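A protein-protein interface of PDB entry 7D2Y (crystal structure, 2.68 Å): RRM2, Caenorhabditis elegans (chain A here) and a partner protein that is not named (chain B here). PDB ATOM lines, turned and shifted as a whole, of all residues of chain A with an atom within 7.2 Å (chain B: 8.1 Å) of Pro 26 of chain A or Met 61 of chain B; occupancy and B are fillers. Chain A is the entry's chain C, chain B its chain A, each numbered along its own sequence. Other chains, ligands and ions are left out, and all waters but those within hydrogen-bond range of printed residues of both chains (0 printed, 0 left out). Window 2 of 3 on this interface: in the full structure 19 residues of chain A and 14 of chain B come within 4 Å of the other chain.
Of the printed residues of chain B, Tyr 27 of chain A touches Lys 38 (3.5 Å) and Met 61 (3.7 Å). Printed residues of chain B within 4 Å of Gln 49 of chain A: Val 39 (3.9 Å), Ser 40 (3.1 Å) and Met 61 (3.7 Å). Of the printed residues of chain B, Asp 56 of chain A touches Lys 38. Printed residues of chain A within 4 Å of Lys 38 of chain B: Tyr 27 (3.5 Å), Gln 52 (3.3 Å) and Asp 56 (3.3 Å). Met 61 of chain B touches three residues of chain A. The nearest residue of chain B that does not touch Pro 26 of chain A is Lys 38 of chain B (4.1 Å). The nearest printed residue of chain B that does not touch Gln 52 of chain A is Gly 37 of chain B (4.5 Å).
Of the 18 printed residues of chain B, 5 touch a printed residue of chain A. Hydrophobic or aromatic side chains of chain B that line the printed part of chain A: Phe 30 and Met 61. Of the 14 printed residues of chain A, 6 touch a printed residue of chain B. Hydrophobic or aromatic side chains of chain A that line the printed part of chain B: Pro 26, Tyr 27 and Phe 48. Among the printed residues, 11 pairs touch across the chains. Among the printed residues, no Asp or Glu carboxylate lies within 4 Å of a Lys or Arg side-chain nitrogen of the other chain.
Among the printed residues, pairs that only touch across the chains: Pro 26 of chain A with Met 61 of chain B (3.6 Å), Tyr 27 of chain A with Lys 38 of chain B (3.5 Å), Tyr 27 of chain A with Met 61 of chain B (3.7 Å), Phe 48 of chain A with Phe 30 of chain B (3.6 Å), Gln 49 of chain A with Val 39 of chain B (3.9 Å), Gln 49 of chain A with Met 61 of chain B (3.7 Å), Gln 52 of chain A with Phe 30 of chain B (3.8 Å), Gln 52 of chain A with Lys 38 of chain B (3.3 Å) and Asp 56 of chain A with Lys 38 of chain B (3.3 Å).
The backbone carbonyl oxygen (O) of Val 39 of chain B lies within hydrogen-bond range of the side-chain amide nitrogen (NE2) of Gln 52 of chain A, at 2.7 Å. The backbone carbonyl oxygen of Ser 40 of chain B is in hydrogen-bond range of the side-chain amide nitrogen of Gln 49 of chain A, 3.1 Å away.
N of Ser 40 of chain B sits at hydrogen-bond distance from O of Asn 59 of chain B, at 2.8 Å. O of Phe 48 of chain A is in hydrogen-bond range of NE2 of Gln 52 of chain A (2.9 Å). OE1 of Gln 49 of chain A sits at hydrogen-bond distance from N of Arg 28 of chain A, 2.7 Å away. The side-chain hydroxyl of Ser 40 of chain B sits at hydrogen-bond distance from the side-chain sulfur of Met 61 of chain B, 3.1 Å away. N of Met 61 of chain B is in hydrogen-bond range of O of Lys 38 of chain B. O of Met 60 of chain B is in hydrogen-bond range of OG of Ser 40 of chain B (3.3 Å).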
ATOM      1  N   ALA A  21      -1.502  -6.217  -4.128  1.00  0.00           N
ATOM      2  CA  ALA A  21      -2.818  -5.752  -4.576  1.00  0.00           C
ATOM      3  C   ALA A  21      -2.766  -5.270  -6.022  1.00  0.00           C
ATOM      4  O   ALA A  21      -3.685  -5.539  -6.803  1.00  0.00           O
ATOM      5  CB  ALA A  21      -3.349  -4.639  -3.670  1.00  0.00           C
ATOM      6  N   GLN A  22      -1.686  -4.575  -6.395  1.00  0.00           N
ATOM      7  CA  GLN A  22      -1.518  -4.149  -7.780  1.00  0.00           C
ATOM      8  C   GLN A  22      -1.498  -5.341  -8.727  1.00  0.00           C
ATOM      9  O   GLN A  22      -2.052  -5.266  -9.829  1.00  0.00           O
ATOM     10  CB  GLN A  22      -0.253  -3.301  -7.917  1.00  0.00           C
ATOM     11  CG  GLN A  22      -0.424  -1.898  -7.356  1.00  0.00           C
ATOM     12  CD  GLN A  22       0.868  -1.195  -7.055  1.00  0.00           C
ATOM     13  OE1 GLN A  22       1.808  -1.787  -6.526  1.00  0.00           O
ATOM     14  NE2 GLN A  22       0.933   0.078  -7.391  1.00  0.00           N
ATOM     15  N   LEU A  23      -0.887  -6.459  -8.312  1.00  0.00           N
ATOM     16  CA  LEU A  23      -0.914  -7.652  -9.153  1.00  0.00           C
ATOM     17  C   LEU A  23      -2.326  -7.990  -9.571  1.00  0.00           C
ATOM     18  O   LEU A  23      -2.548  -8.452 -10.690  1.00  0.00           O
ATOM     19  CB  LEU A  23      -0.357  -8.871  -8.438  1.00  0.00           C
ATOM     20  CG  LEU A  23       1.101  -9.130  -8.230  1.00  0.00           C
ATOM     21  CD1 LEU A  23       1.148 -10.440  -7.477  1.00  0.00           C
ATOM     22  CD2 LEU A  23       1.841  -9.199  -9.535  1.00  0.00           C
ATOM     23  N   LEU A  24      -3.289  -7.786  -8.678  1.00  0.00           N
ATOM     24  CA  LEU A  24      -4.633  -8.301  -8.850  1.00  0.00           C
ATOM     25  C   LEU A  24      -5.569  -7.319  -9.543  1.00  0.00           C
ATOM     26  O   LEU A  24      -6.778  -7.571  -9.581  1.00  0.00           O
ATOM     27  CB  LEU A  24      -5.191  -8.725  -7.481  1.00  0.00           C
ATOM     28  CG  LEU A  24      -4.401  -9.917  -6.880  1.00  0.00           C
ATOM     29  CD1 LEU A  24      -4.762 -10.235  -5.447  1.00  0.00           C
ATOM     30  CD2 LEU A  24      -4.594 -11.132  -7.763  1.00  0.00           C
ATOM     31  N   THR A  25      -5.053  -6.226 -10.098  1.00  0.00           N
ATOM     32  CA  THR A  25      -5.905  -5.250 -10.766  1.00  0.00           C
ATOM     33  C   THR A  25      -6.735  -5.915 -11.864  1.00  0.00           C
ATOM     34  O   THR A  25      -6.184  -6.679 -12.669  1.00  0.00           O
ATOM     35  CB  THR A  25      -5.048  -4.145 -11.367  1.00  0.00           C
ATOM     36  OG1 THR A  25      -4.331  -3.507 -10.324  1.00  0.00           O
ATOM     37  CG2 THR A  25      -5.877  -3.125 -11.990  1.00  0.00           C
ATOM     38  N   PRO A  26      -8.045  -5.619 -11.971  1.00  0.00           N
ATOM     39  CA  PRO A  26      -8.796  -4.599 -11.230  1.00  0.00           C
ATOM     40  C   PRO A  26      -9.664  -5.093 -10.063  1.00  0.00           C
ATOM     41  O   PRO A  26     -10.496  -4.303  -9.596  1.00  0.00           O
ATOM     42  CB  PRO A  26      -9.692  -4.018 -12.310  1.00  0.00           C
ATOM     43  CG  PRO A  26     -10.017  -5.188 -13.146  1.00  0.00           C
ATOM     44  CD  PRO A  26      -8.823  -6.103 -13.124  1.00  0.00           C
ATOM     45  N   TYR A  27      -9.500  -6.334  -9.616  1.00  0.00           N
ATOM     46  CA  TYR A  27     -10.409  -6.898  -8.618  1.00  0.00           C
ATOM     47  C   TYR A  27     -10.262  -6.220  -7.257  1.00  0.00           C
ATOM     48  O   TYR A  27      -9.192  -5.745  -6.892  1.00  0.00           O
ATOM     49  CB  TYR A  27     -10.157  -8.401  -8.483  1.00  0.00           C
ATOM     50  CG  TYR A  27     -10.374  -9.056  -9.811  1.00  0.00           C
ATOM     51  CD1 TYR A  27     -11.631  -9.076 -10.376  1.00  0.00           C
ATOM     52  CD2 TYR A  27      -9.313  -9.572 -10.536  1.00  0.00           C
ATOM     53  CE1 TYR A  27     -11.847  -9.619 -11.591  1.00  0.00           C
ATOM     54  CE2 TYR A  27      -9.516 -10.134 -11.755  1.00  0.00           C
ATOM     55  CZ  TYR A  27     -10.799 -10.151 -12.281  1.00  0.00           C
ATOM     56  OH  TYR A  27     -11.045 -10.684 -13.517  1.00  0.00           O
ATOM     57  N   ARG A  28     -11.361  -6.164  -6.508  1.00  0.00           N
ATOM     58  CA  ARG A  28     -11.350  -5.487  -5.224  1.00  0.00           C
ATOM     59  C   ARG A  28     -10.681  -6.367  -4.178  1.00  0.00           C
ATOM     60  O   ARG A  28     -11.122  -7.492  -3.920  1.00  0.00           O
ATOM     61  CB  ARG A  28     -12.762  -5.115  -4.776  1.00  0.00           C
ATOM     62  CG  ARG A  28     -12.744  -4.205  -3.533  1.00  0.00           C
ATOM     63  CD  ARG A  28     -14.092  -3.674  -3.226  1.00  0.00           C
ATOM     64  NE  ARG A  28     -14.198  -3.104  -1.879  1.00  0.00           N
ATOM     65  CZ  ARG A  28     -14.019  -1.818  -1.584  1.00  0.00           C
ATOM     66  NH1 ARG A  28     -13.678  -0.957  -2.525  1.00  0.00           N
ATOM     67  NH2 ARG A  28     -14.174  -1.395  -0.339  1.00  0.00           N
ATOM     68  N   VAL A  29      -9.628  -5.848  -3.570  1.00  0.00           N
ATOM     69  CA  VAL A  29      -8.922  -6.526  -2.501  1.00  0.00           C
ATOM     70  C   VAL A  29      -9.400  -5.950  -1.179  1.00  0.00           C
ATOM     71  O   VAL A  29      -9.361  -4.733  -0.979  1.00  0.00           O
ATOM     72  CB  VAL A  29      -7.405  -6.353  -2.662  1.00  0.00           C
ATOM     73  CG1 VAL A  29      -6.696  -6.984  -1.503  1.00  0.00           C
ATOM     74  CG2 VAL A  29      -6.973  -6.962  -3.985  1.00  0.00           C
ATOM     75  N   PHE A  48     -17.113 -14.400  -7.195  1.00  0.00           N
ATOM     76  CA  PHE A  48     -17.020 -14.154  -8.621  1.00  0.00           C
ATOM     77  C   PHE A  48     -15.721 -13.440  -8.957  1.00  0.00           C
ATOM     78  O   PHE A  48     -15.058 -13.757  -9.958  1.00  0.00           O
ATOM     79  CB  PHE A  48     -18.241 -13.370  -9.079  1.00  0.00           C
ATOM     80  CG  PHE A  48     -19.531 -14.100  -8.843  1.00  0.00           C
ATOM     81  CD1 PHE A  48     -19.750 -15.351  -9.417  1.00  0.00           C
ATOM     82  CD2 PHE A  48     -20.521 -13.556  -8.040  1.00  0.00           C
ATOM     83  CE1 PHE A  48     -20.961 -16.043  -9.194  1.00  0.00           C
ATOM     84  CE2 PHE A  48     -21.737 -14.245  -7.821  1.00  0.00           C
ATOM     85  CZ  PHE A  48     -21.950 -15.486  -8.395  1.00  0.00           C
ATOM     86  N   GLN A  49     -15.289 -12.525  -8.102  1.00  0.00           N
ATOM     87  CA  GLN A  49     -13.996 -11.930  -8.387  1.00  0.00           C
ATOM     88  C   GLN A  49     -12.897 -12.938  -8.170  1.00  0.00           C
ATOM     89  O   GLN A  49     -11.951 -12.990  -8.955  1.00  0.00           O
ATOM     90  CB  GLN A  49     -13.798 -10.653  -7.573  1.00  0.00           C
ATOM     91  CG  GLN A  49     -14.823  -9.597  -7.981  1.00  0.00           C
ATOM     92  CD  GLN A  49     -14.485  -8.232  -7.462  1.00  0.00           C
ATOM     93  OE1 GLN A  49     -13.318  -7.872  -7.339  1.00  0.00           O
ATOM     94  NE2 GLN A  49     -15.506  -7.455  -7.146  1.00  0.00           N
ATOM     95  N   GLN A  52     -12.779 -15.166 -11.297  1.00  0.00           N
ATOM     96  CA  GLN A  52     -12.163 -14.469 -12.424  1.00  0.00           C
ATOM     97  C   GLN A  52     -10.663 -14.240 -12.215  1.00  0.00           C
ATOM     98  O   GLN A  52      -9.878 -14.336 -13.166  1.00  0.00           O
ATOM     99  CB  GLN A  52     -12.879 -13.140 -12.641  1.00  0.00           C
ATOM    100  CG  GLN A  52     -14.345 -13.315 -12.945  1.00  0.00           C
ATOM    101  CD  GLN A  52     -15.093 -12.013 -12.943  1.00  0.00           C
ATOM    102  OE1 GLN A  52     -15.245 -11.361 -13.980  1.00  0.00           O
ATOM    103  NE2 GLN A  52     -15.572 -11.617 -11.771  1.00  0.00           N
ATOM    104  N   ASP A  56      -7.783 -15.281 -14.696  1.00  0.00           N
ATOM    105  CA  ASP A  56      -6.938 -14.282 -15.347  1.00  0.00           C
ATOM    106  C   ASP A  56      -5.456 -14.498 -15.069  1.00  0.00           C
ATOM    107  O   ASP A  56      -4.614 -14.244 -15.942  1.00  0.00           O
ATOM    108  CB  ASP A  56      -7.310 -12.880 -14.881  1.00  0.00           C
ATOM    109  CG  ASP A  56      -8.641 -12.420 -15.401  1.00  0.00           C
ATOM    110  OD1 ASP A  56      -9.280 -13.170 -16.174  1.00  0.00           O
ATOM    111  OD2 ASP A  56      -9.046 -11.293 -15.027  1.00  0.00           O
ATOM    112  N   PHE A  57      -5.113 -14.907 -13.847  1.00  0.00           N
ATOM    113  CA  PHE A  57      -3.749 -14.781 -13.359  1.00  0.00           C
ATOM    114  C   PHE A  57      -3.048 -16.109 -13.134  1.00  0.00           C
ATOM    115  O   PHE A  57      -1.816 -16.143 -13.154  1.00  0.00           O
ATOM    116  CB  PHE A  57      -3.712 -13.987 -12.035  1.00  0.00           C
ATOM    117  CG  PHE A  57      -4.328 -12.616 -12.122  1.00  0.00           C
ATOM    118  CD1 PHE A  57      -3.819 -11.668 -12.987  1.00  0.00           C
ATOM    119  CD2 PHE A  57      -5.400 -12.278 -11.317  1.00  0.00           C
ATOM    120  CE1 PHE A  57      -4.367 -10.416 -13.068  1.00  0.00           C
ATOM    121  CE2 PHE A  57      -5.974 -11.023 -11.403  1.00  0.00           C
ATOM    122  CZ  PHE A  57      -5.446 -10.083 -12.283  1.00  0.00           C
ATOM    123  N   LEU B  10     -20.225   1.561  -8.646  1.00  0.00           N
ATOM    124  CA  LEU B  10     -19.547   2.383  -9.632  1.00  0.00           C
ATOM    125  C   LEU B  10     -20.588   2.926 -10.600  1.00  0.00           C
ATOM    126  O   LEU B  10     -21.299   2.152 -11.247  1.00  0.00           O
ATOM    127  CB  LEU B  10     -18.478   1.567 -10.357  1.00  0.00           C
ATOM    128  CG  LEU B  10     -17.742   2.223 -11.527  1.00  0.00           C
ATOM    129  CD1 LEU B  10     -16.878   3.380 -11.073  1.00  0.00           C
ATOM    130  CD2 LEU B  10     -16.933   1.190 -12.270  1.00  0.00           C
ATOM    131  N   ALA B  13     -22.169   1.416 -14.081  1.00  0.00           N
ATOM    132  CA  ALA B  13     -21.599   0.101 -14.304  1.00  0.00           C
ATOM    133  C   ALA B  13     -22.572  -1.042 -14.052  1.00  0.00           C
ATOM    134  O   ALA B  13     -22.280  -2.173 -14.451  1.00  0.00           O
ATOM    135  CB  ALA B  13     -20.363  -0.081 -13.431  1.00  0.00           C
ATOM    136  N   GLY B  14     -23.713  -0.788 -13.409  1.00  0.00           N
ATOM    137  CA  GLY B  14     -24.612  -1.839 -13.000  1.00  0.00           C
ATOM    138  C   GLY B  14     -25.903  -1.904 -13.801  1.00  0.00           C
ATOM    139  O   GLY B  14     -26.252  -0.998 -14.543  1.00  0.00           O
ATOM    140  N   PHE B  30     -24.215 -14.949 -13.640  1.00  0.00           N
ATOM    141  CA  PHE B  30     -22.851 -14.464 -13.797  1.00  0.00           C
ATOM    142  C   PHE B  30     -22.288 -14.831 -15.165  1.00  0.00           C
ATOM    143  O   PHE B  30     -21.790 -13.966 -15.901  1.00  0.00           O
ATOM    144  CB  PHE B  30     -21.978 -15.024 -12.677  1.00  0.00           C
ATOM    145  CG  PHE B  30     -20.513 -14.910 -12.944  1.00  0.00           C
ATOM    146  CD1 PHE B  30     -19.849 -13.717 -12.735  1.00  0.00           C
ATOM    147  CD2 PHE B  30     -19.796 -15.998 -13.409  1.00  0.00           C
ATOM    148  CE1 PHE B  30     -18.510 -13.607 -12.995  1.00  0.00           C
ATOM    149  CE2 PHE B  30     -18.451 -15.891 -13.676  1.00  0.00           C
ATOM    150  CZ  PHE B  30     -17.806 -14.697 -13.467  1.00  0.00           C
ATOM    151  N   GLY B  37     -17.432  -9.143 -20.360  1.00  0.00           N
ATOM    152  CA  GLY B  37     -16.420  -8.447 -19.587  1.00  0.00           C
ATOM    153  C   GLY B  37     -16.425  -8.917 -18.145  1.00  0.00           C
ATOM    154  O   GLY B  37     -17.173  -9.804 -17.754  1.00  0.00           O
ATOM    155  N   LYS B  38     -15.555  -8.293 -17.358  1.00  0.00           N
ATOM    156  CA  LYS B  38     -15.359  -8.698 -15.976  1.00  0.00           C
ATOM    157  C   LYS B  38     -16.529  -8.241 -15.111  1.00  0.00           C
ATOM    158  O   LYS B  38     -17.107  -7.172 -15.327  1.00  0.00           O
ATOM    159  CB  LYS B  38     -14.055  -8.120 -15.446  1.00  0.00           C
ATOM    160  CG  LYS B  38     -12.860  -8.619 -16.208  1.00  0.00           C
ATOM    161  CD  LYS B  38     -11.554  -8.051 -15.691  1.00  0.00           C
ATOM    162  CE  LYS B  38     -10.371  -8.594 -16.487  1.00  0.00           C
ATOM    163  NZ  LYS B  38      -9.962  -7.694 -17.599  1.00  0.00           N
ATOM    164  N   VAL B  39     -16.869  -9.059 -14.110  1.00  0.00           N
ATOM    165  CA  VAL B  39     -18.051  -8.831 -13.287  1.00  0.00           C
ATOM    166  C   VAL B  39     -17.615  -8.555 -11.854  1.00  0.00           C
ATOM    167  O   VAL B  39     -16.743  -9.247 -11.327  1.00  0.00           O
ATOM    168  CB  VAL B  39     -19.030 -10.026 -13.354  1.00  0.00           C
ATOM    169  CG1 VAL B  39     -20.249  -9.765 -12.510  1.00  0.00           C
ATOM    170  CG2 VAL B  39     -19.443 -10.299 -14.787  1.00  0.00           C
ATOM    171  N   SER B  40     -18.229  -7.546 -11.227  1.00  0.00           N
ATOM    172  CA  SER B  40     -17.969  -7.136  -9.845  1.00  0.00           C
ATOM    173  C   SER B  40     -18.910  -7.772  -8.832  1.00  0.00           C
ATOM    174  O   SER B  40     -18.457  -8.302  -7.819  1.00  0.00           O
ATOM    175  CB  SER B  40     -18.102  -5.630  -9.706  1.00  0.00           C
ATOM    176  OG  SER B  40     -16.984  -5.007 -10.261  1.00  0.00           O
ATOM    177  N   TYR B  41     -20.218  -7.643  -9.052  1.00  0.00           N
ATOM    178  CA  TYR B  41     -21.240  -8.174  -8.171  1.00  0.00           C
ATOM    179  C   TYR B  41     -22.273  -8.844  -9.050  1.00  0.00           C
ATOM    180  O   TYR B  41     -22.569  -8.366 -10.145  1.00  0.00           O
ATOM    181  CB  TYR B  41     -21.903  -7.095  -7.303  1.00  0.00           C
ATOM    182  CG  TYR B  41     -20.911  -6.242  -6.551  1.00  0.00           C
ATOM    183  CD1 TYR B  41     -20.302  -5.132  -7.168  1.00  0.00           C
ATOM    184  CD2 TYR B  41     -20.554  -6.536  -5.224  1.00  0.00           C
ATOM    185  CE1 TYR B  41     -19.374  -4.337  -6.490  1.00  0.00           C
ATOM    186  CE2 TYR B  41     -19.618  -5.741  -4.529  1.00  0.00           C
ATOM    187  CZ  TYR B  41     -19.034  -4.646  -5.174  1.00  0.00           C
ATOM    188  OH  TYR B  41     -18.112  -3.866  -4.501  1.00  0.00           O
ATOM    189  N   VAL B  58     -26.565  -7.077 -11.477  1.00  0.00           N
ATOM    190  CA  VAL B  58     -25.222  -7.376 -11.938  1.00  0.00           C
ATOM    191  C   VAL B  58     -24.477  -6.070 -12.079  1.00  0.00           C
ATOM    192  O   VAL B  58     -24.945  -5.157 -12.767  1.00  0.00           O
ATOM    193  CB  VAL B  58     -25.209  -8.131 -13.276  1.00  0.00           C
ATOM    194  CG1 VAL B  58     -23.788  -8.378 -13.689  1.00  0.00           C
ATOM    195  CG2 VAL B  58     -25.954  -9.450 -13.151  1.00  0.00           C
ATOM    196  N   ASN B  59     -23.323  -5.984 -11.432  1.00  0.00           N
ATOM    197  CA  ASN B  59     -22.422  -4.857 -11.592  1.00  0.00           C
ATOM    198  C   ASN B  59     -21.184  -5.330 -12.334  1.00  0.00           C
ATOM    199  O   ASN B  59     -20.615  -6.380 -12.011  1.00  0.00           O
ATOM    200  CB  ASN B  59     -22.042  -4.248 -10.242  1.00  0.00           C
ATOM    201  CG  ASN B  59     -21.792  -2.773 -10.337  1.00  0.00           C
ATOM    202  OD1 ASN B  59     -22.657  -2.014 -10.772  1.00  0.00           O
ATOM    203  ND2 ASN B  59     -20.599  -2.347  -9.939  1.00  0.00           N
ATOM    204  N   MET B  60     -20.788  -4.576 -13.342  1.00  0.00           N
ATOM    205  CA  MET B  60     -19.617  -4.942 -14.106  1.00  0.00           C
ATOM    206  C   MET B  60     -18.388  -4.319 -13.463  1.00  0.00           C
ATOM    207  O   MET B  60     -18.484  -3.386 -12.665  1.00  0.00           O
ATOM    208  CB  MET B  60     -19.767  -4.495 -15.554  1.00  0.00           C
ATOM    209  CG  MET B  60     -21.003  -5.046 -16.229  1.00  0.00           C
ATOM    210  SD  MET B  60     -21.022  -6.841 -16.347  1.00  0.00           S
ATOM    211  CE  MET B  60     -19.717  -7.132 -17.543  1.00  0.00           C
ATOM    212  N   MET B  61     -17.219  -4.861 -13.803  1.00  0.00           N
ATOM    213  CA  MET B  61     -15.997  -4.330 -13.216  1.00  0.00           C
ATOM    214  C   MET B  61     -15.730  -2.883 -13.630  1.00  0.00           C
ATOM    215  O   MET B  61     -15.091  -2.159 -12.863  1.00  0.00           O
ATOM    216  CB  MET B  61     -14.807  -5.220 -13.575  1.00  0.00           C
ATOM    217  CG  MET B  61     -13.595  -4.982 -12.709  1.00  0.00           C
ATOM    218  SD  MET B  61     -13.923  -5.253 -10.958  1.00  0.00           S
ATOM    219  CE  MET B  61     -14.537  -6.927 -10.930  1.00  0.00           C
ATOM    220  N   SER B  62     -16.217  -2.436 -14.798  1.00  0.00           N
ATOM    221  CA  SER B  62     -15.956  -1.074 -15.259  1.00  0.00           C
ATOM    222  C   SER B  62     -17.065  -0.566 -16.191  1.00  0.00           C
ATOM    223  O   SER B  62     -17.859  -1.335 -16.746  1.00  0.00           O
ATOM    224  CB  SER B  62     -14.616  -0.969 -15.982  1.00  0.00           C
ATOM    225  OG  SER B  62     -14.704  -1.529 -17.278  1.00  0.00           O
ATOM    226  N   VAL B  63     -17.111   0.761 -16.345  1.00  0.00           N
ATOM    227  CA  VAL B  63     -18.085   1.359 -17.249  1.00  0.00           C
ATOM    228  C   VAL B  63     -17.896   0.821 -18.658  1.00  0.00           C
ATOM    229  O   VAL B  63     -18.865   0.476 -19.342  1.00  0.00           O
ATOM    230  CB  VAL B  63     -17.987   2.896 -17.224  1.00  0.00           C
ATOM    231  CG1 VAL B  63     -18.716   3.472 -18.406  1.00  0.00           C
ATOM    232  CG2 VAL B  63     -18.576   3.448 -15.933  1.00  0.00           C
ATOM    233  N   ALA B  64     -16.646   0.719 -19.101  1.00  0.00           N
ATOM    234  CA  ALA B  64     -16.370   0.089 -20.386  1.00  0.00           C
ATOM    235  C   ALA B  64     -17.037  -1.283 -20.481  1.00  0.00           C
ATOM    236  O   ALA B  64     -17.673  -1.612 -21.483  1.00  0.00           O
ATOM    237  CB  ALA B  64     -14.857  -0.015 -20.585  1.00  0.00           C
ATOM    238  N   ASP B  65     -16.906  -2.097 -19.433  1.00  0.00           N
ATOM    239  CA  ASP B  65     -17.520  -3.420 -19.437  1.00  0.00           C
ATOM    240  C   ASP B  65     -19.043  -3.326 -19.514  1.00  0.00           C
ATOM    241  O   ASP B  65     -19.681  -4.069 -20.269  1.00  0.00           O
ATOM    242  CB  ASP B  65     -17.084  -4.191 -18.192  1.00  0.00           C
ATOM    243  CG  ASP B  65     -15.632  -4.655 -18.265  1.00  0.00           C
ATOM    244  OD1 ASP B  65     -15.274  -5.331 -19.249  1.00  0.00           O
ATOM    245  OD2 ASP B  65     -14.853  -4.351 -17.337  1.00  0.00           O
ATOM    246  N   ALA B  66     -19.641  -2.415 -18.740  1.00  0.00           N
ATOM    247  CA  ALA B  66     -21.080  -2.202 -18.820  1.00  0.00           C
ATOM    248  C   ALA B  66     -21.503  -1.758 -20.221  1.00  0.00           C
ATOM    249  O   ALA B  66     -22.483  -2.278 -20.771  1.00  0.00           O
ATOM    250  CB  ALA B  66     -21.514  -1.181 -17.770  1.00  0.00           C
